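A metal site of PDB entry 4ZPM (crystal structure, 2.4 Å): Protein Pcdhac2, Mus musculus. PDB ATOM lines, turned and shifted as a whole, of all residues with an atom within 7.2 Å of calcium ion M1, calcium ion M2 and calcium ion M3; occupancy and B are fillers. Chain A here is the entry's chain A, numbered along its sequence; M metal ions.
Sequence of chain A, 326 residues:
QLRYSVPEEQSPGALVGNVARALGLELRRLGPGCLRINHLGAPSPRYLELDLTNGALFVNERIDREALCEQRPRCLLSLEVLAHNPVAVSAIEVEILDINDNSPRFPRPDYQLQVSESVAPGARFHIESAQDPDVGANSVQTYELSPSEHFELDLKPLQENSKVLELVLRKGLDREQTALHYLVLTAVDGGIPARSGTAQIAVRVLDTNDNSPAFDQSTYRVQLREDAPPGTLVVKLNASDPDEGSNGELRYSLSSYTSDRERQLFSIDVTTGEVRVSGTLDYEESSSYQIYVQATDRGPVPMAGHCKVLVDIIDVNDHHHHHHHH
Of the 28 residues printed, 7 come within 4 Å of calcium ion M1. The nearest printed residue that does not touch calcium ion M1 is Arg 65 (4.6 Å).
Calcium ion M3 is bound by O of Asn 102 (2.3 Å), OD1 of Asn 100 (2.3 Å), O of Asn 138 (2.4 Å), OD2 of Asp 132 (2.5 Å), OD2 of Asp 134 (2.6 Å), OD2 of Asp 189 (2.8 Å) and OD1 of Asp 132 (2.9 Å).
Calcium ion M2 is bound by the side-chain carboxylate (OD1) of Asp 64 (2.3 Å), the side-chain carboxylate (OE2) of Glu 66 (2.4 Å), the side-chain carboxylate (OD2) of Asp 101 (2.4 Å), the side-chain carboxylate (OE1) of Glu 8 (2.5 Å) and the side-chain carboxylate (OE2) of Glu 9 (2.7 Å).
Calcium ion M1 is bound by the side-chain carboxylate (OD1) of Asp 101 (2.3 Å), the side-chain carboxylate (OD1) of Asp 98 (2.4 Å), the side-chain carboxylate (OE1) of Glu 66 (2.4 Å), the backbone carbonyl oxygen (O) of Ile 99 (2.5 Å), the side-chain carboxylate (OE2) of Glu 8 (2.5 Å), the side-chain carboxylate (OE2) of Glu 66 (2.6 Å) and the side-chain carboxylate (OD1) of Asp 134 (2.7 Å).
The side-chain carboxylate of Glu 9 lies within salt-bridge range of the guanidinium group of Arg 62 (2.9 Å). The side-chain hydroxyl (OG) of Ser 139 sits at hydrogen-bond distance from the backbone carbonyl oxygen (O) of Asp 132 (3.3 Å). ND2 of Asn 138 lies within hydrogen-bond range of OD2 of Asp 98, at 2.6 Å. The backbone carbonyl oxygen of Asn 100 is in hydrogen-bond range of the guanidinium group of Arg 195 (3.2 Å). The backbone NH (N) of Ala 67 sits at hydrogen-bond distance from the side-chain carboxylate (OD2) of Asp 64. The side-chain carboxylate (OD2) of Asp 64 is in salt-bridge range of the guanidinium group (NH2) of Arg 62 (3.9 Å). The side-chain carboxylate of Glu 66 sits close to the guanidinium group of Arg 65. The side-chain carboxylate (OE1) of Glu 8 lies close to the backbone NH (N) of Arg 65, at 3.0 Å.
Six residues have an atom within 4 Å of calcium ion M3: Asn 100, Asn 102, Asp 132, Asp 134, Asn 138 and Asp 189. Along chain A the residues within 4 Å of calcium ion M3 span positions 100 to 189. The nearest printed residue that does not touch calcium ion M3 is Ser 103 (4.4 Å).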
ATOM      1  N   GLU A   8      10.449 -24.540  -0.666  1.00  0.00           N
ATOM      2  CA  GLU A   8       9.428 -23.982  -1.544  1.00  0.00           C
ATOM      3  C   GLU A   8       8.174 -24.871  -1.594  1.00  0.00           C
ATOM      4  O   GLU A   8       8.221 -26.038  -1.196  1.00  0.00           O
ATOM      5  CB  GLU A   8       9.989 -23.790  -2.952  1.00  0.00           C
ATOM      6  CG  GLU A   8      10.290 -25.099  -3.656  1.00  0.00           C
ATOM      7  CD  GLU A   8      10.777 -24.915  -5.082  1.00  0.00           C
ATOM      8  OE1 GLU A   8      10.107 -24.194  -5.857  1.00  0.00           O
ATOM      9  OE2 GLU A   8      11.829 -25.499  -5.430  1.00  0.00           O
ATOM     10  N   GLU A   9       7.080 -24.291  -2.056  1.00  0.00           N
ATOM     11  CA  GLU A   9       5.855 -25.027  -2.400  1.00  0.00           C
ATOM     12  C   GLU A   9       5.148 -25.694  -1.218  1.00  0.00           C
ATOM     13  O   GLU A   9       4.328 -26.591  -1.425  1.00  0.00           O
ATOM     14  CB  GLU A   9       6.182 -26.103  -3.457  1.00  0.00           C
ATOM     15  CG  GLU A   9       6.814 -25.567  -4.737  1.00  0.00           C
ATOM     16  CD  GLU A   9       5.842 -24.786  -5.610  1.00  0.00           C
ATOM     17  OE1 GLU A   9       4.637 -24.757  -5.282  1.00  0.00           O
ATOM     18  OE2 GLU A   9       6.300 -24.196  -6.612  1.00  0.00           O
ATOM     19  N   ARG A  62       1.620 -19.717  -1.716  1.00  0.00           N
ATOM     20  CA  ARG A  62       2.503 -20.619  -2.444  1.00  0.00           C
ATOM     21  C   ARG A  62       3.789 -19.904  -2.825  1.00  0.00           C
ATOM     22  O   ARG A  62       3.770 -18.850  -3.475  1.00  0.00           O
ATOM     23  CB  ARG A  62       1.811 -21.168  -3.697  1.00  0.00           C
ATOM     24  CG  ARG A  62       2.774 -21.839  -4.681  1.00  0.00           C
ATOM     25  CD  ARG A  62       2.090 -22.115  -6.012  1.00  0.00           C
ATOM     26  NE  ARG A  62       2.888 -22.988  -6.864  1.00  0.00           N
ATOM     27  CZ  ARG A  62       3.490 -22.588  -7.985  1.00  0.00           C
ATOM     28  NH1 ARG A  62       3.380 -21.330  -8.387  1.00  0.00           N
ATOM     29  NH2 ARG A  62       4.208 -23.452  -8.696  1.00  0.00           N
ATOM     30  N   ILE A  63       4.919 -20.476  -2.426  1.00  0.00           N
ATOM     31  CA  ILE A  63       6.230 -19.922  -2.728  1.00  0.00           C
ATOM     32  C   ILE A  63       6.941 -20.786  -3.756  1.00  0.00           C
ATOM     33  O   ILE A  63       7.412 -21.873  -3.424  1.00  0.00           O
ATOM     34  CB  ILE A  63       7.088 -19.798  -1.460  1.00  0.00           C
ATOM     35  CG1 ILE A  63       6.330 -19.048  -0.355  1.00  0.00           C
ATOM     36  CG2 ILE A  63       8.420 -19.121  -1.770  1.00  0.00           C
ATOM     37  CD1 ILE A  63       7.172 -18.741   0.862  1.00  0.00           C
ATOM     38  N   ASP A  64       7.015 -20.324  -4.998  1.00  0.00           N
ATOM     39  CA  ASP A  64       7.691 -21.065  -6.080  1.00  0.00           C
ATOM     40  C   ASP A  64       9.075 -20.492  -6.353  1.00  0.00           C
ATOM     41  O   ASP A  64       9.203 -19.414  -6.943  1.00  0.00           O
ATOM     42  CB  ASP A  64       6.846 -21.036  -7.356  1.00  0.00           C
ATOM     43  CG  ASP A  64       7.548 -21.674  -8.555  1.00  0.00           C
ATOM     44  OD1 ASP A  64       8.344 -22.609  -8.360  1.00  0.00           O
ATOM     45  OD2 ASP A  64       7.285 -21.236  -9.699  1.00  0.00           O
ATOM     46  N   ARG A  65      10.104 -21.215  -5.925  1.00  0.00           N
ATOM     47  CA  ARG A  65      11.485 -20.750  -6.075  1.00  0.00           C
ATOM     48  C   ARG A  65      11.873 -20.544  -7.532  1.00  0.00           C
ATOM     49  O   ARG A  65      12.640 -19.631  -7.850  1.00  0.00           O
ATOM     50  CB  ARG A  65      12.449 -21.742  -5.422  1.00  0.00           C
ATOM     51  CG  ARG A  65      13.867 -21.191  -5.275  1.00  0.00           C
ATOM     52  CD  ARG A  65      14.912 -22.278  -5.472  1.00  0.00           C
ATOM     53  NE  ARG A  65      14.817 -22.890  -6.793  1.00  0.00           N
ATOM     54  CZ  ARG A  65      15.305 -22.349  -7.904  1.00  0.00           C
ATOM     55  NH1 ARG A  65      15.926 -21.173  -7.849  1.00  0.00           N
ATOM     56  NH2 ARG A  65      15.171 -22.969  -9.074  1.00  0.00           N
ATOM     57  N   GLU A  66      11.338 -21.371  -8.421  1.00  0.00           N
ATOM     58  CA  GLU A  66      11.633 -21.263  -9.841  1.00  0.00           C
ATOM     59  C   GLU A  66      11.171 -19.929 -10.411  1.00  0.00           C
ATOM     60  O   GLU A  66      11.884 -19.288 -11.182  1.00  0.00           O
ATOM     61  CB  GLU A  66      11.012 -22.419 -10.626  1.00  0.00           C
ATOM     62  CG  GLU A  66      11.844 -23.709 -10.626  1.00  0.00           C
ATOM     63  CD  GLU A  66      11.858 -24.413  -9.289  1.00  0.00           C
ATOM     64  OE1 GLU A  66      12.930 -24.495  -8.650  1.00  0.00           O
ATOM     65  OE2 GLU A  66      10.794 -24.914  -8.866  1.00  0.00           O
ATOM     66  N   ALA A  67       9.966 -19.501 -10.036  1.00  0.00           N
ATOM     67  CA  ALA A  67       9.440 -18.222 -10.490  1.00  0.00           C
ATOM     68  C   ALA A  67      10.192 -17.054  -9.861  1.00  0.00           C
ATOM     69  O   ALA A  67      10.443 -16.045 -10.520  1.00  0.00           O
ATOM     70  CB  ALA A  67       7.958 -18.121 -10.189  1.00  0.00           C
ATOM     71  N   LEU A  97      14.478 -22.837   0.119  1.00  0.00           N
ATOM     72  CA  LEU A  97      15.180 -24.040  -0.315  1.00  0.00           C
ATOM     73  C   LEU A  97      14.524 -24.614  -1.560  1.00  0.00           C
ATOM     74  O   LEU A  97      13.315 -24.535  -1.725  1.00  0.00           O
ATOM     75  CB  LEU A  97      15.195 -25.092   0.799  1.00  0.00           C
ATOM     76  CG  LEU A  97      15.722 -24.655   2.165  1.00  0.00           C
ATOM     77  CD1 LEU A  97      15.655 -25.803   3.155  1.00  0.00           C
ATOM     78  CD2 LEU A  97      17.139 -24.123   2.043  1.00  0.00           C
ATOM     79  N   ASP A  98      15.349 -25.165  -2.446  1.00  0.00           N
ATOM     80  CA  ASP A  98      14.827 -25.773  -3.655  1.00  0.00           C
ATOM     81  C   ASP A  98      14.447 -27.230  -3.434  1.00  0.00           C
ATOM     82  O   ASP A  98      15.180 -27.965  -2.786  1.00  0.00           O
ATOM     83  CB  ASP A  98      15.848 -25.669  -4.794  1.00  0.00           C
ATOM     84  CG  ASP A  98      15.412 -26.405  -6.038  1.00  0.00           C
ATOM     85  OD1 ASP A  98      14.447 -25.939  -6.684  1.00  0.00           O
ATOM     86  OD2 ASP A  98      16.035 -27.428  -6.377  1.00  0.00           O
ATOM     87  N   ILE A  99      13.298 -27.619  -3.958  1.00  0.00           N
ATOM     88  CA  ILE A  99      12.911 -29.027  -3.973  1.00  0.00           C
ATOM     89  C   ILE A  99      12.911 -29.532  -5.409  1.00  0.00           C
ATOM     90  O   ILE A  99      12.885 -28.738  -6.361  1.00  0.00           O
ATOM     91  CB  ILE A  99      11.527 -29.257  -3.331  1.00  0.00           C
ATOM     92  CG1 ILE A  99      10.421 -28.650  -4.197  1.00  0.00           C
ATOM     93  CG2 ILE A  99      11.494 -28.688  -1.920  1.00  0.00           C
ATOM     94  CD1 ILE A  99       9.021 -28.858  -3.637  1.00  0.00           C
ATOM     95  N   ASN A 100      12.951 -30.849  -5.568  1.00  0.00           N
ATOM     96  CA  ASN A 100      12.983 -31.455  -6.894  1.00  0.00           C
ATOM     97  C   ASN A 100      11.602 -31.629  -7.492  1.00  0.00           C
ATOM     98  O   ASN A 100      11.139 -32.751  -7.692  1.00  0.00           O
ATOM     99  CB  ASN A 100      13.696 -32.809  -6.833  1.00  0.00           C
ATOM    100  CG  ASN A 100      14.233 -33.239  -8.181  1.00  0.00           C
ATOM    101  OD1 ASN A 100      14.638 -32.396  -8.980  1.00  0.00           O
ATOM    102  ND2 ASN A 100      14.235 -34.540  -8.439  1.00  0.00           N
ATOM    103  N   ASP A 101      10.931 -30.513  -7.782  1.00  0.00           N
ATOM    104  CA  ASP A 101       9.567 -30.567  -8.287  1.00  0.00           C
ATOM    105  C   ASP A 101       9.503 -30.318  -9.791  1.00  0.00           C
ATOM    106  O   ASP A 101       8.443 -30.038 -10.344  1.00  0.00           O
ATOM    107  CB  ASP A 101       8.677 -29.557  -7.537  1.00  0.00           C
ATOM    108  CG  ASP A 101       9.222 -28.140  -7.605  1.00  0.00           C
ATOM    109  OD1 ASP A 101      10.445 -27.975  -7.805  1.00  0.00           O
ATOM    110  OD2 ASP A 101       8.424 -27.191  -7.429  1.00  0.00           O
ATOM    111  N   ASN A 102      10.649 -30.420 -10.449  1.00  0.00           N
ATOM    112  CA  ASN A 102      10.708 -30.312 -11.903  1.00  0.00           C
ATOM    113  C   ASN A 102      11.549 -31.428 -12.515  1.00  0.00           C
ATOM    114  O   ASN A 102      12.542 -31.858 -11.931  1.00  0.00           O
ATOM    115  CB  ASN A 102      11.257 -28.950 -12.332  1.00  0.00           C
ATOM    116  CG  ASN A 102      10.325 -27.810 -11.979  1.00  0.00           C
ATOM    117  OD1 ASN A 102       9.442 -27.453 -12.758  1.00  0.00           O
ATOM    118  ND2 ASN A 102      10.520 -27.243 -10.801  1.00  0.00           N
ATOM    119  N   SER A 103      11.139 -31.897 -13.690  1.00  0.00           N
ATOM    120  CA  SER A 103      11.873 -32.933 -14.392  1.00  0.00           C
ATOM    121  C   SER A 103      12.718 -32.354 -15.524  1.00  0.00           C
ATOM    122  O   SER A 103      12.362 -31.320 -16.089  1.00  0.00           O
ATOM    123  CB  SER A 103      10.902 -33.985 -14.946  1.00  0.00           C
ATOM    124  OG  SER A 103      10.413 -34.818 -13.918  1.00  0.00           O
ATOM    125  N   PRO A 104      13.842 -33.005 -15.838  1.00  0.00           N
ATOM    126  CA  PRO A 104      14.656 -32.641 -17.002  1.00  0.00           C
ATOM    127  C   PRO A 104      13.858 -32.697 -18.301  1.00  0.00           C
ATOM    128  O   PRO A 104      13.106 -33.648 -18.508  1.00  0.00           O
ATOM    129  CB  PRO A 104      15.768 -33.694 -16.997  1.00  0.00           C
ATOM    130  CG  PRO A 104      15.906 -34.053 -15.568  1.00  0.00           C
ATOM    131  CD  PRO A 104      14.493 -34.060 -15.047  1.00  0.00           C
ATOM    132  N   ASP A 132      16.747 -28.354 -16.852  1.00  0.00           N
ATOM    133  CA  ASP A 132      15.998 -28.585 -15.613  1.00  0.00           C
ATOM    134  C   ASP A 132      15.955 -27.303 -14.788  1.00  0.00           C
ATOM    135  O   ASP A 132      16.967 -26.846 -14.283  1.00  0.00           O
ATOM    136  CB  ASP A 132      16.630 -29.721 -14.794  1.00  0.00           C
ATOM    137  CG  ASP A 132      15.722 -30.220 -13.677  1.00  0.00           C
ATOM    138  OD1 ASP A 132      15.055 -29.400 -13.006  1.00  0.00           O
ATOM    139  OD2 ASP A 132      15.675 -31.446 -13.459  1.00  0.00           O
ATOM    140  N   PRO A 133      14.748 -26.713 -14.668  1.00  0.00           N
ATOM    141  CA  PRO A 133      14.600 -25.418 -13.995  1.00  0.00           C
ATOM    142  C   PRO A 133      14.968 -25.440 -12.504  1.00  0.00           C
ATOM    143  O   PRO A 133      15.063 -24.375 -11.899  1.00  0.00           O
ATOM    144  CB  PRO A 133      13.108 -25.092 -14.189  1.00  0.00           C
ATOM    145  CG  PRO A 133      12.451 -26.399 -14.466  1.00  0.00           C
ATOM    146  CD  PRO A 133      13.474 -27.233 -15.187  1.00  0.00           C
ATOM    147  N   ASP A 134      15.183 -26.619 -11.930  1.00  0.00           N
ATOM    148  CA  ASP A 134      15.652 -26.709 -10.552  1.00  0.00           C
ATOM    149  C   ASP A 134      17.130 -26.316 -10.493  1.00  0.00           C
ATOM    150  O   ASP A 134      17.741 -26.024 -11.518  1.00  0.00           O
ATOM    151  CB  ASP A 134      15.459 -28.107  -9.974  1.00  0.00           C
ATOM    152  CG  ASP A 134      14.004 -28.495  -9.848  1.00  0.00           C
ATOM    153  OD1 ASP A 134      13.128 -27.614  -9.978  1.00  0.00           O
ATOM    154  OD2 ASP A 134      13.728 -29.689  -9.624  1.00  0.00           O
ATOM    155  N   VAL A 135      17.697 -26.320  -9.287  1.00  0.00           N
ATOM    156  CA  VAL A 135      19.074 -25.882  -9.084  1.00  0.00           C
ATOM    157  C   VAL A 135      19.849 -26.891  -8.256  1.00  0.00           C
ATOM    158  O   VAL A 135      19.264 -27.751  -7.597  1.00  0.00           O
ATOM    159  CB  VAL A 135      19.139 -24.496  -8.389  1.00  0.00           C
ATOM    160  CG1 VAL A 135      18.601 -23.411  -9.318  1.00  0.00           C
ATOM    161  CG2 VAL A 135      18.379 -24.525  -7.071  1.00  0.00           C
ATOM    162  N   ALA A 137      21.801 -30.030  -6.963  1.00  0.00           N
ATOM    163  CA  ALA A 137      21.655 -31.461  -7.208  1.00  0.00           C
ATOM    164  C   ALA A 137      20.346 -31.791  -7.924  1.00  0.00           C
ATOM    165  O   ALA A 137      20.256 -32.777  -8.645  1.00  0.00           O
ATOM    166  CB  ALA A 137      21.743 -32.226  -5.902  1.00  0.00           C
ATOM    167  N   ASN A 138      19.335 -30.962  -7.711  1.00  0.00           N
ATOM    168  CA  ASN A 138      18.021 -31.190  -8.310  1.00  0.00           C
ATOM    169  C   ASN A 138      17.992 -30.949  -9.822  1.00  0.00           C
ATOM    170  O   ASN A 138      16.999 -31.262 -10.484  1.00  0.00           O
ATOM    171  CB  ASN A 138      16.974 -30.317  -7.630  1.00  0.00           C
ATOM    172  CG  ASN A 138      16.705 -30.736  -6.201  1.00  0.00           C
ATOM    173  OD1 ASN A 138      16.890 -31.887  -5.826  1.00  0.00           O
ATOM    174  ND2 ASN A 138      16.261 -29.785  -5.380  1.00  0.00           N
ATOM    175  N   SER A 139      19.062 -30.391 -10.368  1.00  0.00           N
ATOM    176  CA  SER A 139      19.152 -30.151 -11.799  1.00  0.00           C
ATOM    177  C   SER A 139      19.776 -31.343 -12.517  1.00  0.00           C
ATOM    178  O   SER A 139      20.160 -32.319 -11.876  1.00  0.00           O
ATOM    179  CB  SER A 139      19.957 -28.869 -12.085  1.00  0.00           C
ATOM    180  OG  SER A 139      19.703 -28.399 -13.397  1.00  0.00           O
ATOM    181  N   VAL A 140      19.895 -31.249 -13.841  1.00  0.00           N
ATOM    182  CA  VAL A 140      20.440 -32.357 -14.639  1.00  0.00           C
ATOM    183  C   VAL A 140      21.875 -32.716 -14.249  1.00  0.00           C
ATOM    184  O   VAL A 140      22.749 -31.852 -14.212  1.00  0.00           O
ATOM    185  CB  VAL A 140      20.399 -32.030 -16.127  1.00  0.00           C
ATOM    186  CG1 VAL A 140      21.010 -33.160 -16.945  1.00  0.00           C
ATOM    187  CG2 VAL A 140      18.966 -31.755 -16.563  1.00  0.00           C
ATOM    188  N   ASP A 189      18.215 -36.161 -13.117  1.00  0.00           N
ATOM    189  CA  ASP A 189      18.698 -35.230 -12.097  1.00  0.00           C
ATOM    190  C   ASP A 189      19.218 -35.995 -10.888  1.00  0.00           C
ATOM    191  O   ASP A 189      19.135 -37.223 -10.840  1.00  0.00           O
ATOM    192  CB  ASP A 189      17.621 -34.209 -11.692  1.00  0.00           C
ATOM    193  CG  ASP A 189      16.363 -34.836 -11.087  1.00  0.00           C
ATOM    194  OD1 ASP A 189      16.443 -35.872 -10.379  1.00  0.00           O
ATOM    195  OD2 ASP A 189      15.274 -34.268 -11.309  1.00  0.00           O
ATOM    196  N   GLY A 190      19.745 -35.276  -9.904  1.00  0.00           N
ATOM    197  CA  GLY A 190      20.337 -35.893  -8.733  1.00  0.00           C
ATOM    198  C   GLY A 190      19.451 -35.888  -7.510  1.00  0.00           C
ATOM    199  O   GLY A 190      19.898 -36.201  -6.401  1.00  0.00           O
ATOM    200  N   GLY A 191      18.189 -35.527  -7.698  1.00  0.00           N
ATOM    201  CA  GLY A 191      17.213 -35.580  -6.625  1.00  0.00           C
ATOM    202  C   GLY A 191      16.895 -37.013  -6.242  1.00  0.00           C
ATOM    203  O   GLY A 191      17.143 -37.928  -7.019  1.00  0.00           O
ATOM    204  N   ARG A 195      14.405 -37.784 -11.112  1.00  0.00           N
ATOM    205  CA  ARG A 195      13.402 -37.510 -12.137  1.00  0.00           C
ATOM    206  C   ARG A 195      14.073 -37.493 -13.512  1.00  0.00           C
ATOM    207  O   ARG A 195      15.224 -37.069 -13.654  1.00  0.00           O
ATOM    208  CB  ARG A 195      12.687 -36.194 -11.856  1.00  0.00           C
ATOM    209  CG  ARG A 195      11.964 -36.193 -10.514  1.00  0.00           C
ATOM    210  CD  ARG A 195      11.260 -34.869 -10.238  1.00  0.00           C
ATOM    211  NE  ARG A 195      10.266 -34.556 -11.252  1.00  0.00           N
ATOM    212  CZ  ARG A 195       9.127 -33.910 -11.012  1.00  0.00           C
ATOM    213  NH1 ARG A 195       8.845 -33.510  -9.778  1.00  0.00           N
ATOM    214  NH2 ARG A 195       8.275 -33.670 -12.000  1.00  0.00           N
HETATM  215 CA    CA M   1      12.360 -26.637  -7.633  1.00  0.00          CA
HETATM  216 CA    CA M   2       8.639 -24.815  -7.819  1.00  0.00          CA
HETATM  217 CA    CA M   3      14.697 -31.562 -11.169  1.00  0.00          CA
